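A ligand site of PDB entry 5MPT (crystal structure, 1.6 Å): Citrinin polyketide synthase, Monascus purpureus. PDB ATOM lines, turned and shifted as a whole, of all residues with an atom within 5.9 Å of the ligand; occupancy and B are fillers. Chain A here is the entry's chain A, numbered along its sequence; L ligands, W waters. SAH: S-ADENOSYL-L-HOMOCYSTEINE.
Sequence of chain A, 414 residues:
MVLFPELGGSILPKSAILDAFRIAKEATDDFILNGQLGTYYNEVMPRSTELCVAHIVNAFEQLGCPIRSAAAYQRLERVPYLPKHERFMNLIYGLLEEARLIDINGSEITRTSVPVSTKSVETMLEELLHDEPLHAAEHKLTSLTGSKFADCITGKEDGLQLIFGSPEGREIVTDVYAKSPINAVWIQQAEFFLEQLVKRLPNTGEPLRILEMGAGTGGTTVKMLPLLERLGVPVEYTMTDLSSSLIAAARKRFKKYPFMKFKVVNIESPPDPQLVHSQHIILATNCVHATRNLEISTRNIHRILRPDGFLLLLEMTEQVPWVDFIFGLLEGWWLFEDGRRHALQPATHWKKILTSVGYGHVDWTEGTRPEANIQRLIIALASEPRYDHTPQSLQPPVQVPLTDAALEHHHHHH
The backbone carbonyl oxygen (O) of Ala 215 lies close to an oxygen (OXT) of the ligand (3.3 Å).
Gly 216 touches the ligand (CA to O3', 3.1 Å).
Gly 218 touches the ligand (N to OXT, 3.8 Å).
CD1 of Leu 246 touches O3' of the ligand, 3.999 Å away.
Val 265 touches the ligand (O to C2, 3.3 Å).
Asn 286 touches the ligand (O to CG, 3.4 Å).
CB of Cys 287 touches O4' of the ligand, 3.2 Å away.
Within 4 Å of the ligand: Tyr 177, Gly 214, Ala 215, Gly 216, Thr 217, Gly 218, Gly 219, Asp 241, Leu 242, Leu 246, Val 265, Asn 266, Ile 267, Thr 285, Asn 286 and Cys 287.
O3' of the ligand sits at hydrogen-bond distance from OD1 of Asp 241.
O of the ligand sits at hydrogen-bond distance from N of Thr 217 (2.7 Å).
The side-chain hydroxyl (OG1) of Thr 217 sits at hydrogen-bond distance from an oxygen (O) of the ligand, 2.7 Å away.
A nitrogen (N) of the ligand is in hydrogen-bond range of the backbone carbonyl oxygen (O) of Gly 214, 2.8 Å away.
A nitrogen (N6) of the ligand is in hydrogen-bond range of the side-chain amide oxygen (OD1) of Asn 266.
O of Thr 285 is in hydrogen-bond range of N of the ligand (2.9 Å).
The backbone NH (N) of Gly 219 is in hydrogen-bond range of an oxygen (OXT) of the ligand, at 3.0 Å.
The backbone NH (N) of Ile 267 is in hydrogen-bond range of a nitrogen (N1) of the ligand (3.0 Å).
N of Leu 242 sits at hydrogen-bond distance from N3 of the ligand, 3.3 Å away.
A sulfur (SD) of the ligand sits close to the side-chain hydroxyl of Tyr 177, at 3.5 Å.
Water W1 lies within hydrogen-bond range of O of the ligand and N of Thr 217.
Water W4 lies within hydrogen-bond range of O of Ala 290 and N7 of the ligand.
Water W6 bridges the side-chain carboxylate of Glu 268 (2.9 Å) and a nitrogen (N6) of the ligand (2.9 Å).
Water W2 lies within hydrogen-bond range of the side-chain carboxylate (OE2) of Glu 212, the backbone carbonyl oxygen (O) of Ala 215, the backbone NH (N) of Thr 220, an oxygen (OXT) of the ligand, the side-chain hydroxyl (OG1) of Thr 221 and the backbone NH (N) of Gly 219.
Water W3 lies within hydrogen-bond range of the side-chain hydroxyl (OG1) of Thr 240 (2.7 Å), the backbone carbonyl oxygen (O) of Val 265 (2.9 Å), the backbone NH (N) of Gly 214 (3.0 Å) and the backbone NH (N) of Asp 241 (3.3 Å).
The side-chain carboxylate of Asp 241 is in hydrogen-bond range of the backbone NH of Gly 216, at 2.7 Å.
N of Ala 215 sits at hydrogen-bond distance from OD1 of Asp 241.
N of Val 265 sits at hydrogen-bond distance from O of Asp 241 (3.0 Å).
OD2 of Asp 241 is in hydrogen-bond range of N of Ser 243, at 2.8 Å.
The side-chain amide oxygen of Asn 266 sits at hydrogen-bond distance from the backbone NH of Glu 268 (2.8 Å).
The side-chain sulfur of Cys 287 is in hydrogen-bond range of the backbone carbonyl oxygen of Met 213 (3.5 Å).
The backbone carbonyl oxygen (O) of Thr 240 is in hydrogen-bond range of the backbone NH (N) of Ala 215, at 2.9 Å.
The backbone NH (N) of Leu 246 is in hydrogen-bond range of the side-chain hydroxyl (OG) of Ser 243, at 3.1 Å.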
ATOM      1  N   TYR A 177     -17.745  15.429  11.107  1.00  0.00           N
ATOM      2  CA  TYR A 177     -18.624  16.516  11.531  1.00  0.00           C
ATOM      3  C   TYR A 177     -18.077  17.901  11.241  1.00  0.00           C
ATOM      4  O   TYR A 177     -18.869  18.822  11.082  1.00  0.00           O
ATOM      5  CB  TYR A 177     -18.929  16.403  13.038  1.00  0.00           C
ATOM      6  CG  TYR A 177     -19.801  15.235  13.445  1.00  0.00           C
ATOM      7  CD1 TYR A 177     -20.927  14.865  12.721  1.00  0.00           C
ATOM      8  CD2 TYR A 177     -19.494  14.518  14.576  1.00  0.00           C
ATOM      9  CE1 TYR A 177     -21.714  13.840  13.126  1.00  0.00           C
ATOM     10  CE2 TYR A 177     -20.273  13.493  14.985  1.00  0.00           C
ATOM     11  CZ  TYR A 177     -21.383  13.148  14.251  1.00  0.00           C
ATOM     12  OH  TYR A 177     -22.150  12.100  14.726  1.00  0.00           O
ATOM     13  N   GLU A 212     -25.385  26.739  22.034  1.00  0.00           N
ATOM     14  CA  GLU A 212     -25.312  25.634  21.084  1.00  0.00           C
ATOM     15  C   GLU A 212     -25.735  24.350  21.785  1.00  0.00           C
ATOM     16  O   GLU A 212     -25.161  23.977  22.813  1.00  0.00           O
ATOM     17  CB  GLU A 212     -23.910  25.510  20.492  1.00  0.00           C
ATOM     18  CG  GLU A 212     -23.834  24.388  19.473  1.00  0.00           C
ATOM     19  CD  GLU A 212     -22.477  24.195  18.865  1.00  0.00           C
ATOM     20  OE1 GLU A 212     -21.516  24.869  19.280  1.00  0.00           O
ATOM     21  OE2 GLU A 212     -22.374  23.314  17.985  1.00  0.00           O
ATOM     22  N   MET A 213     -26.749  23.706  21.234  1.00  0.00           N
ATOM     23  CA  MET A 213     -27.173  22.409  21.710  1.00  0.00           C
ATOM     24  C   MET A 213     -26.546  21.313  20.870  1.00  0.00           C
ATOM     25  O   MET A 213     -26.224  21.502  19.702  1.00  0.00           O
ATOM     26  CB  MET A 213     -28.688  22.289  21.674  1.00  0.00           C
ATOM     27  CG  MET A 213     -29.335  23.332  22.556  1.00  0.00           C
ATOM     28  SD  MET A 213     -31.108  23.140  22.644  1.00  0.00           S
ATOM     29  CE  MET A 213     -31.429  23.708  24.307  1.00  0.00           C
ATOM     30  N   GLY A 214     -26.349  20.170  21.510  1.00  0.00           N
ATOM     31  CA  GLY A 214     -25.785  19.019  20.812  1.00  0.00           C
ATOM     32  C   GLY A 214     -24.456  19.339  20.149  1.00  0.00           C
ATOM     33  O   GLY A 214     -24.140  18.810  19.075  1.00  0.00           O
ATOM     34  N   ALA A 215     -23.647  20.161  20.805  1.00  0.00           N
ATOM     35  CA  ALA A 215     -22.429  20.653  20.182  1.00  0.00           C
ATOM     36  C   ALA A 215     -21.425  19.527  19.970  1.00  0.00           C
ATOM     37  O   ALA A 215     -20.558  19.637  19.084  1.00  0.00           O
ATOM     38  CB  ALA A 215     -21.812  21.754  21.041  1.00  0.00           C
ATOM     39  N   GLY A 216     -21.530  18.457  20.738  1.00  0.00           N
ATOM     40  CA  GLY A 216     -20.769  17.262  20.519  1.00  0.00           C
ATOM     41  C   GLY A 216     -19.287  17.476  20.355  1.00  0.00           C
ATOM     42  O   GLY A 216     -18.627  18.002  21.270  1.00  0.00           O
ATOM     43  N   THR A 217     -18.770  17.091  19.194  1.00  0.00           N
ATOM     44  CA  THR A 217     -17.357  17.139  18.838  1.00  0.00           C
ATOM     45  C   THR A 217     -16.887  18.539  18.477  1.00  0.00           C
ATOM     46  O   THR A 217     -15.691  18.737  18.255  1.00  0.00           O
ATOM     47  CB  THR A 217     -17.061  16.181  17.674  1.00  0.00           C
ATOM     48  OG1 THR A 217     -17.764  16.578  16.483  1.00  0.00           O
ATOM     49  CG2 THR A 217     -17.417  14.717  18.039  1.00  0.00           C
ATOM     50  N   GLY A 218     -17.794  19.518  18.442  1.00  0.00           N
ATOM     51  CA  GLY A 218     -17.422  20.872  18.099  1.00  0.00           C
ATOM     52  C   GLY A 218     -17.262  21.099  16.617  1.00  0.00           C
ATOM     53  O   GLY A 218     -16.460  21.958  16.220  1.00  0.00           O
ATOM     54  N   GLY A 219     -18.014  20.372  15.784  1.00  0.00           N
ATOM     55  CA  GLY A 219     -17.865  20.524  14.351  1.00  0.00           C
ATOM     56  C   GLY A 219     -18.328  21.890  13.885  1.00  0.00           C
ATOM     57  O   GLY A 219     -17.761  22.478  12.961  1.00  0.00           O
ATOM     58  N   THR A 220     -19.361  22.403  14.539  1.00  0.00           N
ATOM     59  CA  THR A 220     -19.807  23.764  14.334  1.00  0.00           C
ATOM     60  C   THR A 220     -19.046  24.719  15.235  1.00  0.00           C
ATOM     61  O   THR A 220     -18.638  25.799  14.788  1.00  0.00           O
ATOM     62  CB  THR A 220     -21.317  23.846  14.605  1.00  0.00           C
ATOM     63  OG1 THR A 220     -22.015  22.971  13.708  1.00  0.00           O
ATOM     64  CG2 THR A 220     -21.822  25.272  14.441  1.00  0.00           C
ATOM     65  N   THR A 221     -18.849  24.323  16.475  1.00  0.00           N
ATOM     66  CA  THR A 221     -18.213  25.187  17.467  1.00  0.00           C
ATOM     67  C   THR A 221     -16.857  25.668  16.988  1.00  0.00           C
ATOM     68  O   THR A 221     -16.496  26.841  17.203  1.00  0.00           O
ATOM     69  CB  THR A 221     -18.072  24.431  18.778  1.00  0.00           C
ATOM     70  OG1 THR A 221     -19.217  23.580  18.968  1.00  0.00           O
ATOM     71  CG2 THR A 221     -17.933  25.400  19.939  1.00  0.00           C
ATOM     72  N   THR A 240     -23.081  23.398  24.737  1.00  0.00           N
ATOM     73  CA  THR A 240     -23.729  22.363  25.534  1.00  0.00           C
ATOM     74  C   THR A 240     -23.905  21.074  24.742  1.00  0.00           C
ATOM     75  O   THR A 240     -23.826  21.044  23.514  1.00  0.00           O
ATOM     76  CB  THR A 240     -25.095  22.838  26.050  1.00  0.00           C
ATOM     77  OG1 THR A 240     -26.090  22.696  25.024  1.00  0.00           O
ATOM     78  CG2 THR A 240     -25.049  24.296  26.501  1.00  0.00           C
ATOM     79  N   ASP A 241     -24.154  19.981  25.484  1.00  0.00           N
ATOM     80  CA  ASP A 241     -24.393  18.672  24.891  1.00  0.00           C
ATOM     81  C   ASP A 241     -24.938  17.775  25.990  1.00  0.00           C
ATOM     82  O   ASP A 241     -24.778  18.070  27.172  1.00  0.00           O
ATOM     83  CB  ASP A 241     -23.128  18.028  24.305  1.00  0.00           C
ATOM     84  CG  ASP A 241     -23.430  16.892  23.311  1.00  0.00           C
ATOM     85  OD1 ASP A 241     -23.510  17.108  22.082  1.00  0.00           O
ATOM     86  OD2 ASP A 241     -23.570  15.749  23.755  1.00  0.00           O
ATOM     87  N   LEU A 242     -25.572  16.691  25.577  1.00  0.00           N
ATOM     88  CA  LEU A 242     -25.967  15.660  26.518  1.00  0.00           C
ATOM     89  C   LEU A 242     -24.761  14.998  27.167  1.00  0.00           C
ATOM     90  O   LEU A 242     -24.859  14.540  28.307  1.00  0.00           O
ATOM     91  CB  LEU A 242     -26.820  14.608  25.816  1.00  0.00           C
ATOM     92  CG  LEU A 242     -27.531  13.611  26.768  1.00  0.00           C
ATOM     93  CD1 LEU A 242     -28.481  14.319  27.711  1.00  0.00           C
ATOM     94  CD2 LEU A 242     -28.319  12.600  25.963  1.00  0.00           C
ATOM     95  N   SER A 243     -23.636  14.913  26.453  1.00  0.00           N
ATOM     96  CA  SER A 243     -22.467  14.136  26.890  1.00  0.00           C
ATOM     97  C   SER A 243     -21.525  14.988  27.739  1.00  0.00           C
ATOM     98  O   SER A 243     -20.996  15.995  27.266  1.00  0.00           O
ATOM     99  CB  SER A 243     -21.722  13.589  25.680  1.00  0.00           C
ATOM    100  OG  SER A 243     -20.387  13.259  26.003  1.00  0.00           O
ATOM    101  N   LEU A 246     -17.774  14.841  26.275  1.00  0.00           N
ATOM    102  CA  LEU A 246     -17.547  15.762  25.151  1.00  0.00           C
ATOM    103  C   LEU A 246     -17.442  17.204  25.622  1.00  0.00           C
ATOM    104  O   LEU A 246     -16.640  17.970  25.088  1.00  0.00           O
ATOM    105  CB  LEU A 246     -18.662  15.612  24.117  1.00  0.00           C
ATOM    106  CG  LEU A 246     -18.636  14.284  23.333  1.00  0.00           C
ATOM    107  CD1 LEU A 246     -19.796  14.168  22.357  1.00  0.00           C
ATOM    108  CD2 LEU A 246     -17.327  14.127  22.560  1.00  0.00           C
ATOM    109  N   VAL A 265     -26.519  19.919  28.812  1.00  0.00           N
ATOM    110  CA  VAL A 265     -27.919  20.299  28.647  1.00  0.00           C
ATOM    111  C   VAL A 265     -28.609  19.245  27.793  1.00  0.00           C
ATOM    112  O   VAL A 265     -28.117  18.893  26.717  1.00  0.00           O
ATOM    113  CB  VAL A 265     -28.096  21.690  28.012  1.00  0.00           C
ATOM    114  CG1 VAL A 265     -29.585  21.952  27.706  1.00  0.00           C
ATOM    115  CG2 VAL A 265     -27.519  22.752  28.905  1.00  0.00           C
ATOM    116  N   ASN A 266     -29.741  18.755  28.259  1.00  0.00           N
ATOM    117  CA  ASN A 266     -30.551  17.785  27.533  1.00  0.00           C
ATOM    118  C   ASN A 266     -31.687  18.517  26.832  1.00  0.00           C
ATOM    119  O   ASN A 266     -32.508  19.172  27.503  1.00  0.00           O
ATOM    120  CB  ASN A 266     -31.082  16.732  28.495  1.00  0.00           C
ATOM    121  CG  ASN A 266     -31.840  15.618  27.811  1.00  0.00           C
ATOM    122  OD1 ASN A 266     -32.298  15.742  26.678  1.00  0.00           O
ATOM    123  ND2 ASN A 266     -32.045  14.538  28.555  1.00  0.00           N
ATOM    124  N   ILE A 267     -31.676  18.480  25.501  1.00  0.00           N
ATOM    125  CA  ILE A 267     -32.707  19.090  24.662  1.00  0.00           C
ATOM    126  C   ILE A 267     -34.095  18.694  25.087  1.00  0.00           C
ATOM    127  O   ILE A 267     -35.034  19.495  24.959  1.00  0.00           O
ATOM    128  CB  ILE A 267     -32.456  18.727  23.192  1.00  0.00           C
ATOM    129  CG1 ILE A 267     -31.109  19.287  22.744  1.00  0.00           C
ATOM    130  CG2 ILE A 267     -33.615  19.178  22.287  1.00  0.00           C
ATOM    131  CD1 ILE A 267     -30.544  18.670  21.453  1.00  0.00           C
ATOM    132  N   GLU A 268     -34.263  17.450  25.589  1.00  0.00           N
ATOM    133  CA  GLU A 268     -35.601  16.944  25.932  1.00  0.00           C
ATOM    134  C   GLU A 268     -36.101  17.470  27.260  1.00  0.00           C
ATOM    135  O   GLU A 268     -37.306  17.386  27.530  1.00  0.00           O
ATOM    136  CB  GLU A 268     -35.606  15.409  25.976  1.00  0.00           C
ATOM    137  CG  GLU A 268     -35.308  14.785  24.632  1.00  0.00           C
ATOM    138  CD  GLU A 268     -35.603  13.294  24.555  1.00  0.00           C
ATOM    139  OE1 GLU A 268     -36.211  12.746  25.508  1.00  0.00           O
ATOM    140  OE2 GLU A 268     -35.213  12.686  23.542  1.00  0.00           O
ATOM    141  N   THR A 285     -26.918  21.585  15.456  1.00  0.00           N
ATOM    142  CA  THR A 285     -26.494  20.885  14.243  1.00  0.00           C
ATOM    143  C   THR A 285     -26.696  19.395  14.454  1.00  0.00           C
ATOM    144  O   THR A 285     -25.962  18.771  15.213  1.00  0.00           O
ATOM    145  CB  THR A 285     -25.037  21.207  13.927  1.00  0.00           C
ATOM    146  OG1 THR A 285     -24.931  22.600  13.649  1.00  0.00           O
ATOM    147  CG2 THR A 285     -24.504  20.348  12.758  1.00  0.00           C
ATOM    148  N   ASN A 286     -27.726  18.860  13.758  1.00  0.00           N
ATOM    149  CA  ASN A 286     -28.008  17.430  13.630  1.00  0.00           C
ATOM    150  C   ASN A 286     -28.092  16.731  14.973  1.00  0.00           C
ATOM    151  O   ASN A 286     -27.662  15.583  15.147  1.00  0.00           O
ATOM    152  CB  ASN A 286     -26.996  16.781  12.694  1.00  0.00           C
ATOM    153  CG  ASN A 286     -27.423  16.974  11.266  1.00  0.00           C
ATOM    154  OD1 ASN A 286     -28.590  16.730  10.919  1.00  0.00           O
ATOM    155  ND2 ASN A 286     -26.534  17.455  10.431  1.00  0.00           N
ATOM    156  N   CYS A 287     -28.719  17.398  15.914  1.00  0.00           N
ATOM    157  CA  CYS A 287     -28.983  16.832  17.219  1.00  0.00           C
ATOM    158  C   CYS A 287     -30.461  16.797  17.568  1.00  0.00           C
ATOM    159  O   CYS A 287     -30.891  15.863  18.251  1.00  0.00           O
ATOM    160  CB  CYS A 287     -28.226  17.603  18.311  1.00  0.00           C
ATOM    161  SG  CYS A 287     -28.657  19.369  18.335  1.00  0.00           S
ATOM    162  N   ALA A 290     -32.430  13.697  16.880  1.00  0.00           N
ATOM    163  CA  ALA A 290     -32.109  12.491  17.653  1.00  0.00           C
ATOM    164  C   ALA A 290     -32.950  12.354  18.892  1.00  0.00           C
ATOM    165  O   ALA A 290     -32.810  11.351  19.601  1.00  0.00           O
ATOM    166  CB  ALA A 290     -30.620  12.503  18.059  1.00  0.00           C
ATOM    167  N   THR A 291     -33.826  13.298  19.136  1.00  0.00           N
ATOM    168  CA  THR A 291     -34.640  13.251  20.337  1.00  0.00           C
ATOM    169  C   THR A 291     -35.934  12.475  20.080  1.00  0.00           C
ATOM    170  O   THR A 291     -36.307  12.187  18.933  1.00  0.00           O
ATOM    171  CB  THR A 291     -34.948  14.655  20.856  1.00  0.00           C
ATOM    172  OG1 THR A 291     -35.782  15.379  19.938  1.00  0.00           O
ATOM    173  CG2 THR A 291     -33.668  15.447  21.093  1.00  0.00           C
ATOM    174  N   PHE A 327     -24.988   5.117  11.116  1.00  0.00           N
ATOM    175  CA  PHE A 327     -25.691   5.566  12.300  1.00  0.00           C
ATOM    176  C   PHE A 327     -26.874   4.695  12.621  1.00  0.00           C
ATOM    177  O   PHE A 327     -27.276   4.629  13.800  1.00  0.00           O
ATOM    178  CB  PHE A 327     -26.103   7.020  12.128  1.00  0.00           C
ATOM    179  CG  PHE A 327     -24.954   7.974  12.195  1.00  0.00           C
ATOM    180  CD1 PHE A 327     -24.231   8.307  11.071  1.00  0.00           C
ATOM    181  CD2 PHE A 327     -24.616   8.580  13.400  1.00  0.00           C
ATOM    182  CE1 PHE A 327     -23.158   9.185  11.137  1.00  0.00           C
ATOM    183  CE2 PHE A 327     -23.558   9.477  13.470  1.00  0.00           C
ATOM    184  CZ  PHE A 327     -22.824   9.774  12.351  1.00  0.00           C
HETATM  185  N   SAH L   1     -23.282  18.812  16.443  1.00  0.00           N
HETATM  186  CA  SAH L   1     -22.590  17.491  16.444  1.00  0.00           C
HETATM  187  CB  SAH L   1     -22.884  16.534  15.293  1.00  0.00           C
HETATM  188  CG  SAH L   1     -24.239  15.853  15.371  1.00  0.00           C
HETATM  189  SD  SAH L   1     -24.044  14.426  16.499  1.00  0.00           S
HETATM  190  C   SAH L   1     -21.054  17.764  16.446  1.00  0.00           C
HETATM  191  O   SAH L   1     -20.377  16.789  17.007  1.00  0.00           O
HETATM  192  OXT SAH L   1     -20.543  18.737  15.946  1.00  0.00           O
HETATM  193  C5' SAH L   1     -25.461  14.612  17.614  1.00  0.00           C
HETATM  194  C4' SAH L   1     -25.005  15.241  18.913  1.00  0.00           C
HETATM  195  O4' SAH L   1     -26.205  15.467  19.670  1.00  0.00           O
HETATM  196  C3' SAH L   1     -24.090  14.371  19.781  1.00  0.00           C
HETATM  197  O3' SAH L   1     -23.037  15.213  20.261  1.00  0.00           O
HETATM  198  C2' SAH L   1     -25.015  13.893  20.910  1.00  0.00           C
HETATM  199  O2' SAH L   1     -24.336  13.710  22.147  1.00  0.00           O
HETATM  200  C1' SAH L   1     -25.988  15.059  20.999  1.00  0.00           C
HETATM  201  N9  SAH L   1     -27.286  14.757  21.585  1.00  0.00           N
HETATM  202  C8  SAH L   1     -28.069  13.649  21.406  1.00  0.00           C
HETATM  203  N7  SAH L   1     -29.174  13.651  22.111  1.00  0.00           N
HETATM  204  C5  SAH L   1     -29.115  14.837  22.815  1.00  0.00           C
HETATM  205  C6  SAH L   1     -29.994  15.434  23.744  1.00  0.00           C
HETATM  206  N6  SAH L   1     -31.121  14.869  24.185  1.00  0.00           N
HETATM  207  N1  SAH L   1     -29.636  16.637  24.252  1.00  0.00           N
HETATM  208  C2  SAH L   1     -28.487  17.198  23.854  1.00  0.00           C
HETATM  209  N3  SAH L   1     -27.586  16.733  22.977  1.00  0.00           N
HETATM  210  C4  SAH L   1     -27.968  15.537  22.491  1.00  0.00           C
HETATM  211  O   HOH W   1     -20.900  14.534  18.542  1.00  0.00           O
HETATM  212  O   HOH W   2     -20.673  21.618  17.050  1.00  0.00           O
HETATM  213  O   HOH W   3     -27.204  20.339  24.374  1.00  0.00           O
HETATM  214  O   HOH W   4     -30.984  11.424  21.743  1.00  0.00           O
HETATM  215  O   HOH W   5     -24.676  21.596  17.363  1.00  0.00           O
HETATM  216  O   HOH W   6     -32.376  12.286  23.815  1.00  0.00           O
